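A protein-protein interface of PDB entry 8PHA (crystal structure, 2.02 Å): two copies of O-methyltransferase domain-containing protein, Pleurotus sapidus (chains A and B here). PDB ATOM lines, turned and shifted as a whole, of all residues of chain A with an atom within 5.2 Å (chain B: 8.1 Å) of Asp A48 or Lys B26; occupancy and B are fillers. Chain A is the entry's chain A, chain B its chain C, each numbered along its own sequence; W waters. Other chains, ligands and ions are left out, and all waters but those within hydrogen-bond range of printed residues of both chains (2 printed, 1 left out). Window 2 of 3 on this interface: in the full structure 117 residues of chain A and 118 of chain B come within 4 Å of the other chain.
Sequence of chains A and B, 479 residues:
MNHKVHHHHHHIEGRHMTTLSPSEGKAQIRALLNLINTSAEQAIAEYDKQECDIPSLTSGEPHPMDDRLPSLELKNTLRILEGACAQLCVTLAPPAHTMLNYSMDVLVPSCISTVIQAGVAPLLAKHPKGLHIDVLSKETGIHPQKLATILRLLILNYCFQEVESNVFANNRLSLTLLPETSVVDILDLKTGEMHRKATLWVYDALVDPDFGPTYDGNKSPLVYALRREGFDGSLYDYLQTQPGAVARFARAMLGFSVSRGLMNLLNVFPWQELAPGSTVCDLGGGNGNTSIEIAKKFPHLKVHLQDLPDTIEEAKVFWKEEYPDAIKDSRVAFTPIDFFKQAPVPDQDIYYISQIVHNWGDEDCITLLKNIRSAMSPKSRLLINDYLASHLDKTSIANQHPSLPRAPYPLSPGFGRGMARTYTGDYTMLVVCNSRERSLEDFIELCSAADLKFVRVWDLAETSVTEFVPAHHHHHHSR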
ATOM      1  N   ILE A  44      11.359  -2.674  23.135  1.00  0.00           N
ATOM      2  CA  ILE A  44      10.467  -1.521  23.163  1.00  0.00           C
ATOM      3  C   ILE A  44      11.126  -0.362  23.903  1.00  0.00           C
ATOM      4  O   ILE A  44      11.104   0.780  23.429  1.00  0.00           O
ATOM      5  CB  ILE A  44       9.117  -1.892  23.802  1.00  0.00           C
ATOM      6  CG1 ILE A  44       8.357  -2.918  22.952  1.00  0.00           C
ATOM      7  CG2 ILE A  44       8.276  -0.631  23.988  1.00  0.00           C
ATOM      8  CD1 ILE A  44       6.974  -3.260  23.514  1.00  0.00           C
ATOM      9  N   ALA A  45      11.761  -0.645  25.047  1.00  0.00           N
ATOM     10  CA  ALA A  45      12.448   0.415  25.787  1.00  0.00           C
ATOM     11  C   ALA A  45      13.533   1.064  24.940  1.00  0.00           C
ATOM     12  O   ALA A  45      13.771   2.273  25.038  1.00  0.00           O
ATOM     13  CB  ALA A  45      13.050  -0.134  27.080  1.00  0.00           C
ATOM     14  N   GLU A  46      14.215   0.275  24.111  1.00  0.00           N
ATOM     15  CA  GLU A  46      15.232   0.850  23.237  1.00  0.00           C
ATOM     16  C   GLU A  46      14.601   1.785  22.210  1.00  0.00           C
ATOM     17  O   GLU A  46      15.197   2.804  21.831  1.00  0.00           O
ATOM     18  CB  GLU A  46      16.024  -0.259  22.544  1.00  0.00           C
ATOM     19  CG  GLU A  46      16.967  -0.973  23.475  1.00  0.00           C
ATOM     20  CD  GLU A  46      17.826  -0.020  24.284  1.00  0.00           C
ATOM     21  OE1 GLU A  46      18.505   0.846  23.680  1.00  0.00           O
ATOM     22  OE2 GLU A  46      17.808  -0.131  25.528  1.00  0.00           O
ATOM     23  N   TYR A  47      13.401   1.452  21.733  1.00  0.00           N
ATOM     24  CA  TYR A  47      12.735   2.382  20.821  1.00  0.00           C
ATOM     25  C   TYR A  47      12.269   3.642  21.562  1.00  0.00           C
ATOM     26  O   TYR A  47      12.434   4.761  21.058  1.00  0.00           O
ATOM     27  CB  TYR A  47      11.579   1.684  20.093  1.00  0.00           C
ATOM     28  CG  TYR A  47      12.091   0.798  18.974  1.00  0.00           C
ATOM     29  CD1 TYR A  47      12.463   1.335  17.745  1.00  0.00           C
ATOM     30  CD2 TYR A  47      12.270  -0.567  19.170  1.00  0.00           C
ATOM     31  CE1 TYR A  47      12.972   0.527  16.725  1.00  0.00           C
ATOM     32  CE2 TYR A  47      12.768  -1.381  18.163  1.00  0.00           C
ATOM     33  CZ  TYR A  47      13.122  -0.830  16.947  1.00  0.00           C
ATOM     34  OH  TYR A  47      13.621  -1.648  15.958  1.00  0.00           O
ATOM     35  N   ASP A  48      11.751   3.485  22.785  1.00  0.00           N
ATOM     36  CA  ASP A  48      11.320   4.636  23.582  1.00  0.00           C
ATOM     37  C   ASP A  48      12.487   5.564  23.919  1.00  0.00           C
ATOM     38  O   ASP A  48      12.313   6.788  23.965  1.00  0.00           O
ATOM     39  CB  ASP A  48      10.641   4.167  24.873  1.00  0.00           C
ATOM     40  CG  ASP A  48       9.180   3.756  24.661  1.00  0.00           C
ATOM     41  OD1 ASP A  48       8.623   4.018  23.574  1.00  0.00           O
ATOM     42  OD2 ASP A  48       8.593   3.156  25.590  1.00  0.00           O
ATOM     43  N   LYS A  49      13.681   5.009  24.148  1.00  0.00           N
ATOM     44  CA  LYS A  49      14.827   5.840  24.519  1.00  0.00           C
ATOM     45  C   LYS A  49      15.149   6.862  23.444  1.00  0.00           C
ATOM     46  O   LYS A  49      15.631   7.955  23.755  1.00  0.00           O
ATOM     47  CB  LYS A  49      16.054   4.974  24.796  1.00  0.00           C
ATOM     48  CG  LYS A  49      16.100   4.388  26.200  1.00  0.00           C
ATOM     49  CD  LYS A  49      17.317   3.477  26.367  1.00  0.00           C
ATOM     50  CE  LYS A  49      17.057   2.389  27.401  1.00  0.00           C
ATOM     51  NZ  LYS A  49      18.268   1.552  27.664  1.00  0.00           N
ATOM     52  N   GLN A  50      14.921   6.522  22.179  1.00  0.00           N
ATOM     53  CA  GLN A  50      15.112   7.455  21.078  1.00  0.00           C
ATOM     54  C   GLN A  50      13.811   8.138  20.686  1.00  0.00           C
ATOM     55  O   GLN A  50      13.723   8.709  19.593  1.00  0.00           O
ATOM     56  CB  GLN A  50      15.735   6.742  19.876  1.00  0.00           C
ATOM     57  CG  GLN A  50      17.254   6.570  19.998  1.00  0.00           C
ATOM     58  CD  GLN A  50      17.880   5.978  18.752  1.00  0.00           C
ATOM     59  OE1 GLN A  50      18.055   6.665  17.741  1.00  0.00           O
ATOM     60  NE2 GLN A  50      18.208   4.690  18.810  1.00  0.00           N
ATOM     61  N   GLU A  51      12.794   8.065  21.551  1.00  0.00           N
ATOM     62  CA  GLU A  51      11.500   8.696  21.312  1.00  0.00           C
ATOM     63  C   GLU A  51      10.912   8.254  19.976  1.00  0.00           C
ATOM     64  O   GLU A  51      10.393   9.060  19.202  1.00  0.00           O
ATOM     65  CB  GLU A  51      11.599  10.219  21.398  1.00  0.00           C
ATOM     66  CG  GLU A  51      11.674  10.744  22.826  1.00  0.00           C
ATOM     67  CD  GLU A  51      11.753  12.261  22.884  1.00  0.00           C
ATOM     68  OE1 GLU A  51      12.768  12.828  22.424  1.00  0.00           O
ATOM     69  OE2 GLU A  51      10.784  12.885  23.375  1.00  0.00           O
ATOM     70  N   CYS A  52      10.999   6.957  19.697  1.00  0.00           N
ATOM     71  CA  CYS A  52      10.455   6.402  18.473  1.00  0.00           C
ATOM     72  C   CYS A  52       9.332   5.435  18.804  1.00  0.00           C
ATOM     73  O   CYS A  52       9.354   4.755  19.836  1.00  0.00           O
ATOM     74  CB  CYS A  52      11.532   5.681  17.643  1.00  0.00           C
ATOM     75  SG  CYS A  52      12.691   6.797  16.840  1.00  0.00           S
ATOM     76  N   ASP A  53       8.347   5.388  17.919  1.00  0.00           N
ATOM     77  CA  ASP A  53       7.317   4.380  18.048  1.00  0.00           C
ATOM     78  C   ASP A  53       7.841   3.064  17.487  1.00  0.00           C
ATOM     79  O   ASP A  53       8.926   2.993  16.891  1.00  0.00           O
ATOM     80  CB  ASP A  53       6.036   4.822  17.335  1.00  0.00           C
ATOM     81  CG  ASP A  53       4.780   4.099  17.859  1.00  0.00           C
ATOM     82  OD1 ASP A  53       4.896   3.242  18.770  1.00  0.00           O
ATOM     83  OD2 ASP A  53       3.671   4.410  17.372  1.00  0.00           O
ATOM     84  N   ILE A  54       7.062   2.010  17.712  1.00  0.00           N
ATOM     85  CA  ILE A  54       7.382   0.691  17.166  1.00  0.00           C
ATOM     86  C   ILE A  54       7.440   0.776  15.646  1.00  0.00           C
ATOM     87  O   ILE A  54       6.564   1.413  15.026  1.00  0.00           O
ATOM     88  CB  ILE A  54       6.332  -0.335  17.621  1.00  0.00           C
ATOM     89  CG1 ILE A  54       6.153  -0.291  19.148  1.00  0.00           C
ATOM     90  CG2 ILE A  54       6.696  -1.727  17.134  1.00  0.00           C
ATOM     91  CD1 ILE A  54       7.411  -0.518  19.949  1.00  0.00           C
ATOM     92  N   HIS B  16       6.244  -2.851  32.029  1.00  0.00           N
ATOM     93  CA  HIS B  16       5.304  -1.781  31.727  1.00  0.00           C
ATOM     94  C   HIS B  16       5.578  -1.118  30.382  1.00  0.00           C
ATOM     95  O   HIS B  16       4.892  -0.151  30.032  1.00  0.00           O
ATOM     96  CB  HIS B  16       5.337  -0.725  32.839  1.00  0.00           C
ATOM     97  CG  HIS B  16       5.234  -1.300  34.218  1.00  0.00           C
ATOM     98  ND1 HIS B  16       4.256  -2.201  34.578  1.00  0.00           N
ATOM     99  CD2 HIS B  16       5.990  -1.105  35.324  1.00  0.00           C
ATOM    100  CE1 HIS B  16       4.410  -2.536  35.845  1.00  0.00           C
ATOM    101  NE2 HIS B  16       5.455  -1.883  36.323  1.00  0.00           N
ATOM    102  N   MET B  17       6.544  -1.626  29.610  1.00  0.00           N
ATOM    103  CA  MET B  17       6.953  -0.961  28.380  1.00  0.00           C
ATOM    104  C   MET B  17       5.872  -0.994  27.305  1.00  0.00           C
ATOM    105  O   MET B  17       5.866  -0.122  26.429  1.00  0.00           O
ATOM    106  CB  MET B  17       8.240  -1.597  27.851  1.00  0.00           C
ATOM    107  CG  MET B  17       9.401  -1.572  28.843  1.00  0.00           C
ATOM    108  SD  MET B  17       9.788   0.090  29.440  1.00  0.00           S
ATOM    109  CE  MET B  17       9.050   0.060  31.081  1.00  0.00           C
ATOM    110  N   THR B  18       4.953  -1.958  27.354  1.00  0.00           N
ATOM    111  CA  THR B  18       3.848  -1.957  26.405  1.00  0.00           C
ATOM    112  C   THR B  18       2.731  -0.990  26.790  1.00  0.00           C
ATOM    113  O   THR B  18       1.866  -0.719  25.951  1.00  0.00           O
ATOM    114  CB  THR B  18       3.252  -3.366  26.250  1.00  0.00           C
ATOM    115  OG1 THR B  18       2.919  -3.903  27.539  1.00  0.00           O
ATOM    116  CG2 THR B  18       4.230  -4.304  25.552  1.00  0.00           C
ATOM    117  N   THR B  19       2.721  -0.457  28.021  1.00  0.00           N
ATOM    118  CA  THR B  19       1.611   0.370  28.491  1.00  0.00           C
ATOM    119  C   THR B  19       2.001   1.770  28.952  1.00  0.00           C
ATOM    120  O   THR B  19       1.108   2.605  29.139  1.00  0.00           O
ATOM    121  CB  THR B  19       0.875  -0.313  29.658  1.00  0.00           C
ATOM    122  OG1 THR B  19       1.705  -0.283  30.827  1.00  0.00           O
ATOM    123  CG2 THR B  19       0.526  -1.768  29.318  1.00  0.00           C
ATOM    124  N   LEU B  20       3.292   2.055  29.139  1.00  0.00           N
ATOM    125  CA  LEU B  20       3.715   3.335  29.701  1.00  0.00           C
ATOM    126  C   LEU B  20       3.360   4.499  28.779  1.00  0.00           C
ATOM    127  O   LEU B  20       2.715   5.468  29.198  1.00  0.00           O
ATOM    128  CB  LEU B  20       5.219   3.304  29.983  1.00  0.00           C
ATOM    129  CG  LEU B  20       5.715   4.333  30.994  1.00  0.00           C
ATOM    130  CD1 LEU B  20       4.952   4.173  32.293  1.00  0.00           C
ATOM    131  CD2 LEU B  20       7.211   4.186  31.225  1.00  0.00           C
ATOM    132  N   SER B  21       3.803   4.438  27.522  1.00  0.00           N
ATOM    133  CA  SER B  21       3.447   5.421  26.498  1.00  0.00           C
ATOM    134  C   SER B  21       2.698   4.682  25.399  1.00  0.00           C
ATOM    135  O   SER B  21       3.312   4.175  24.449  1.00  0.00           O
ATOM    136  CB  SER B  21       4.684   6.128  25.950  1.00  0.00           C
ATOM    137  OG  SER B  21       4.321   6.990  24.886  1.00  0.00           O
ATOM    138  N   PRO B  22       1.371   4.638  25.462  1.00  0.00           N
ATOM    139  CA  PRO B  22       0.616   3.689  24.637  1.00  0.00           C
ATOM    140  C   PRO B  22       0.584   4.055  23.159  1.00  0.00           C
ATOM    141  O   PRO B  22       0.663   5.223  22.773  1.00  0.00           O
ATOM    142  CB  PRO B  22      -0.788   3.748  25.243  1.00  0.00           C
ATOM    143  CG  PRO B  22      -0.880   5.125  25.818  1.00  0.00           C
ATOM    144  CD  PRO B  22       0.497   5.445  26.329  1.00  0.00           C
ATOM    145  N   SER B  23       0.446   3.025  22.328  1.00  0.00           N
ATOM    146  CA  SER B  23       0.339   3.209  20.887  1.00  0.00           C
ATOM    147  C   SER B  23      -0.254   1.949  20.276  1.00  0.00           C
ATOM    148  O   SER B  23      -0.281   0.886  20.903  1.00  0.00           O
ATOM    149  CB  SER B  23       1.704   3.536  20.262  1.00  0.00           C
ATOM    150  OG  SER B  23       2.540   2.391  20.237  1.00  0.00           O
ATOM    151  N   GLU B  24      -0.719   2.077  19.032  1.00  0.00           N
ATOM    152  CA  GLU B  24      -1.239   0.902  18.340  1.00  0.00           C
ATOM    153  C   GLU B  24      -0.143  -0.134  18.108  1.00  0.00           C
ATOM    154  O   GLU B  24      -0.388  -1.342  18.235  1.00  0.00           O
ATOM    155  CB  GLU B  24      -1.877   1.298  17.013  1.00  0.00           C
ATOM    156  CG  GLU B  24      -2.799   0.226  16.470  1.00  0.00           C
ATOM    157  CD  GLU B  24      -2.923   0.274  14.967  1.00  0.00           C
ATOM    158  OE1 GLU B  24      -1.967   0.743  14.313  1.00  0.00           O
ATOM    159  OE2 GLU B  24      -3.974  -0.153  14.439  1.00  0.00           O
ATOM    160  N   GLY B  25       1.074   0.322  17.781  1.00  0.00           N
ATOM    161  CA  GLY B  25       2.176  -0.609  17.565  1.00  0.00           C
ATOM    162  C   GLY B  25       2.540  -1.387  18.819  1.00  0.00           C
ATOM    163  O   GLY B  25       2.870  -2.580  18.754  1.00  0.00           O
ATOM    164  N   LYS B  26       2.495  -0.723  19.977  1.00  0.00           N
ATOM    165  CA  LYS B  26       2.729  -1.428  21.232  1.00  0.00           C
ATOM    166  C   LYS B  26       1.606  -2.416  21.524  1.00  0.00           C
ATOM    167  O   LYS B  26       1.858  -3.519  22.028  1.00  0.00           O
ATOM    168  CB  LYS B  26       2.883  -0.428  22.379  1.00  0.00           C
ATOM    169  CG  LYS B  26       4.247   0.276  22.393  1.00  0.00           C
ATOM    170  CD  LYS B  26       4.280   1.429  23.387  1.00  0.00           C
ATOM    171  CE  LYS B  26       5.623   2.154  23.338  1.00  0.00           C
ATOM    172  NZ  LYS B  26       5.856   2.997  24.552  1.00  0.00           N
ATOM    173  N   ALA B  27       0.359  -2.050  21.201  1.00  0.00           N
ATOM    174  CA  ALA B  27      -0.736  -2.996  21.382  1.00  0.00           C
ATOM    175  C   ALA B  27      -0.534  -4.226  20.519  1.00  0.00           C
ATOM    176  O   ALA B  27      -0.793  -5.356  20.957  1.00  0.00           O
ATOM    177  CB  ALA B  27      -2.079  -2.338  21.058  1.00  0.00           C
ATOM    178  N   GLN B  28      -0.055  -4.028  19.288  1.00  0.00           N
ATOM    179  CA  GLN B  28       0.185  -5.169  18.422  1.00  0.00           C
ATOM    180  C   GLN B  28       1.329  -6.029  18.949  1.00  0.00           C
ATOM    181  O   GLN B  28       1.248  -7.260  18.900  1.00  0.00           O
ATOM    182  CB  GLN B  28       0.458  -4.699  16.998  1.00  0.00           C
ATOM    183  CG  GLN B  28      -0.743  -4.047  16.335  1.00  0.00           C
ATOM    184  CD  GLN B  28      -0.633  -4.022  14.820  1.00  0.00           C
ATOM    185  OE1 GLN B  28       0.114  -4.796  14.223  1.00  0.00           O
ATOM    186  NE2 GLN B  28      -1.359  -3.114  14.195  1.00  0.00           N
ATOM    187  N   ILE B  29       2.390  -5.411  19.481  1.00  0.00           N
ATOM    188  CA  ILE B  29       3.476  -6.205  20.065  1.00  0.00           C
ATOM    189  C   ILE B  29       2.948  -7.046  21.226  1.00  0.00           C
ATOM    190  O   ILE B  29       3.241  -8.247  21.340  1.00  0.00           O
ATOM    191  CB  ILE B  29       4.636  -5.302  20.521  1.00  0.00           C
ATOM    192  CG1 ILE B  29       5.319  -4.612  19.332  1.00  0.00           C
ATOM    193  CG2 ILE B  29       5.657  -6.120  21.306  1.00  0.00           C
ATOM    194  CD1 ILE B  29       6.118  -5.547  18.430  1.00  0.00           C
ATOM    195  N   ARG B  30       2.163  -6.427  22.111  1.00  0.00           N
ATOM    196  CA  ARG B  30       1.629  -7.178  23.241  1.00  0.00           C
ATOM    197  C   ARG B  30       0.696  -8.291  22.771  1.00  0.00           C
ATOM    198  O   ARG B  30       0.643  -9.371  23.375  1.00  0.00           O
ATOM    199  CB  ARG B  30       0.903  -6.258  24.225  1.00  0.00           C
ATOM    200  CG  ARG B  30       0.134  -7.083  25.232  1.00  0.00           C
ATOM    201  CD  ARG B  30      -0.242  -6.369  26.493  1.00  0.00           C
ATOM    202  NE  ARG B  30      -0.293  -7.325  27.593  1.00  0.00           N
ATOM    203  CZ  ARG B  30      -1.319  -8.126  27.859  1.00  0.00           C
ATOM    204  NH1 ARG B  30      -2.410  -8.133  27.106  1.00  0.00           N
ATOM    205  NH2 ARG B  30      -1.247  -8.942  28.907  1.00  0.00           N
ATOM    206  N   ALA B  31      -0.041  -8.055  21.681  1.00  0.00           N
ATOM    207  CA  ALA B  31      -0.928  -9.098  21.181  1.00  0.00           C
ATOM    208  C   ALA B  31      -0.127 -10.234  20.551  1.00  0.00           C
ATOM    209  O   ALA B  31      -0.522 -11.402  20.649  1.00  0.00           O
ATOM    210  CB  ALA B  31      -1.941  -8.510  20.200  1.00  0.00           C
ATOM    211  N   LEU B  32       1.006  -9.918  19.908  1.00  0.00           N
ATOM    212  CA  LEU B  32       1.890 -10.982  19.437  1.00  0.00           C
ATOM    213  C   LEU B  32       2.405 -11.813  20.605  1.00  0.00           C
ATOM    214  O   LEU B  32       2.441 -13.049  20.535  1.00  0.00           O
ATOM    215  CB  LEU B  32       3.066 -10.398  18.662  1.00  0.00           C
ATOM    216  CG  LEU B  32       2.744  -9.819  17.286  1.00  0.00           C
ATOM    217  CD1 LEU B  32       3.985  -9.136  16.729  1.00  0.00           C
ATOM    218  CD2 LEU B  32       2.271 -10.928  16.358  1.00  0.00           C
ATOM    219  N   LEU B  33       2.815 -11.146  21.685  1.00  0.00           N
ATOM    220  CA  LEU B  33       3.269 -11.859  22.877  1.00  0.00           C
ATOM    221  C   LEU B  33       2.175 -12.758  23.434  1.00  0.00           C
ATOM    222  O   LEU B  33       2.444 -13.882  23.871  1.00  0.00           O
ATOM    223  CB  LEU B  33       3.734 -10.864  23.941  1.00  0.00           C
ATOM    224  CG  LEU B  33       5.073 -10.158  23.681  1.00  0.00           C
ATOM    225  CD1 LEU B  33       5.365  -9.106  24.756  1.00  0.00           C
ATOM    226  CD2 LEU B  33       6.205 -11.166  23.603  1.00  0.00           C
ATOM    227  N   THR B  91       9.600  -7.287  13.385  1.00  0.00           N
ATOM    228  CA  THR B  91       9.176  -5.937  13.758  1.00  0.00           C
ATOM    229  C   THR B  91      10.228  -5.240  14.611  1.00  0.00           C
ATOM    230  O   THR B  91      10.555  -4.069  14.373  1.00  0.00           O
ATOM    231  CB  THR B  91       7.850  -5.992  14.514  1.00  0.00           C
ATOM    232  OG1 THR B  91       6.851  -6.624  13.702  1.00  0.00           O
ATOM    233  CG2 THR B  91       7.364  -4.575  14.891  1.00  0.00           C
ATOM    234  N   TYR B 409      -5.622 -11.850  15.309  1.00  0.00           N
ATOM    235  CA  TYR B 409      -4.984 -10.558  15.519  1.00  0.00           C
ATOM    236  C   TYR B 409      -3.721 -10.727  16.360  1.00  0.00           C
ATOM    237  O   TYR B 409      -3.735 -11.446  17.363  1.00  0.00           O
ATOM    238  CB  TYR B 409      -5.979  -9.620  16.214  1.00  0.00           C
ATOM    239  CG  TYR B 409      -5.439  -8.307  16.734  1.00  0.00           C
ATOM    240  CD1 TYR B 409      -5.234  -7.228  15.880  1.00  0.00           C
ATOM    241  CD2 TYR B 409      -5.203  -8.123  18.093  1.00  0.00           C
ATOM    242  CE1 TYR B 409      -4.767  -6.016  16.370  1.00  0.00           C
ATOM    243  CE2 TYR B 409      -4.727  -6.923  18.585  1.00  0.00           C
ATOM    244  CZ  TYR B 409      -4.513  -5.873  17.725  1.00  0.00           C
ATOM    245  OH  TYR B 409      -4.047  -4.686  18.226  1.00  0.00           O
ATOM    246  N   PRO B 410      -2.608 -10.068  15.995  1.00  0.00           N
ATOM    247  CA  PRO B 410      -2.421  -9.153  14.869  1.00  0.00           C
ATOM    248  C   PRO B 410      -1.592  -9.771  13.738  1.00  0.00           C
ATOM    249  O   PRO B 410      -0.895  -9.051  13.022  1.00  0.00           O
ATOM    250  CB  PRO B 410      -1.667  -7.999  15.529  1.00  0.00           C
ATOM    251  CG  PRO B 410      -0.715  -8.745  16.484  1.00  0.00           C
ATOM    252  CD  PRO B 410      -1.438 -10.033  16.885  1.00  0.00           C
HETATM  253  O   HOH W   1       1.935   2.924  16.565  1.00  0.00           O
HETATM  254  O   HOH W   2      13.017  -2.416  13.053  1.00  0.00           O
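NZ of Lys B26 is in hydrogen-bond range of O of Ser B21, at 2.8 Å.
The backbone NH (N) of Lys B26 is in hydrogen-bond range of the side-chain hydroxyl (OG) of Ser B23 (3.1 Å).
Printed residues of chain B that touch a printed residue of chain A: Met B17, Thr B18, Ser B23, Gly B25, Lys B26, Ile B29 and Thr B91.
Of the 11 printed residues of chain A, 4 touch a printed residue of chain B.
Printed residues of chain A that touch a printed residue of chain B: Ile A44, Asp A48, Asp A53 and Ile A54.
Hydrophobic or aromatic side chains of chain A within 4 Å of the printed part of chain B: Ile A44 and Ile A54.
Among the printed residues, 10 pairs touch across the chains.
Of the printed residues of chain A, Met B17 touches Ile A44 (3.5 Å).
Thr B19 touches none of the printed residues of chain A.
Ser B21 touches none of the printed residues of chain A.
Printed residues of chain A within 4 Å of Ser B23: Asp A53.
Of the printed residues of chain A, Gly B25 touches Ile A54.
Lys B26 touches just these residues of chain A: Ile A44 (3.9 Å), Asp A48 (2.9 Å) and Ile A54 (3.8 Å).
Printed residues of chain A within 4 Å of Ile B29: Ile A44 (3.8 Å) and Ile A54 (3.9 Å).
Of the printed residues of chain A, Thr B91 touches Ile A54 (3.7 Å).
The nearest residue of chain B that does not touch Asp A48 is Met B17 (4.3 Å).
The nearest printed residue of chain A that does not touch Thr B91 is Tyr A47 (4.2 Å).
No position is printed for both chains.
Of the 10 pairs that touch across the chains among the printed residues, none has its exchanged pair printed and touching as well.
The side-chain amino group of Lys B26 lies within salt-bridge range of the side-chain carboxylate of Asp A48, 2.9 Å away.
The side-chain hydroxyl (OG) of Ser B23 is in hydrogen-bond range of the side-chain carboxylate (OD1) of Asp A53.
Ile A44 touches Met B17.
Thr B18 touches Ile A44.
Ile A44 touches Lys B26 (CG2 to CE, 3.9 Å).
Ile A44 touches Ile B29.
CG1 of Ile A54 touches C of Gly B25, at 3.8 Å.
CG1 of Ile A54 touches N of Lys B26, at 3.8 Å.
CG2 of Ile A54 touches CG1 of Ile B29 (3.9 Å).
Thr B91 touches Ile A54 (CG2 to CG2, 3.7 Å).
Water W1 lies within hydrogen-bond range of the side-chain carboxylate (OD2) of Asp A53 (2.4 Å) and the backbone NH (N) of Gly B25 (3.0 Å).
Water W2 bridges OH of Tyr A47 (3.1 Å) and O of Thr B91 (3.2 Å).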
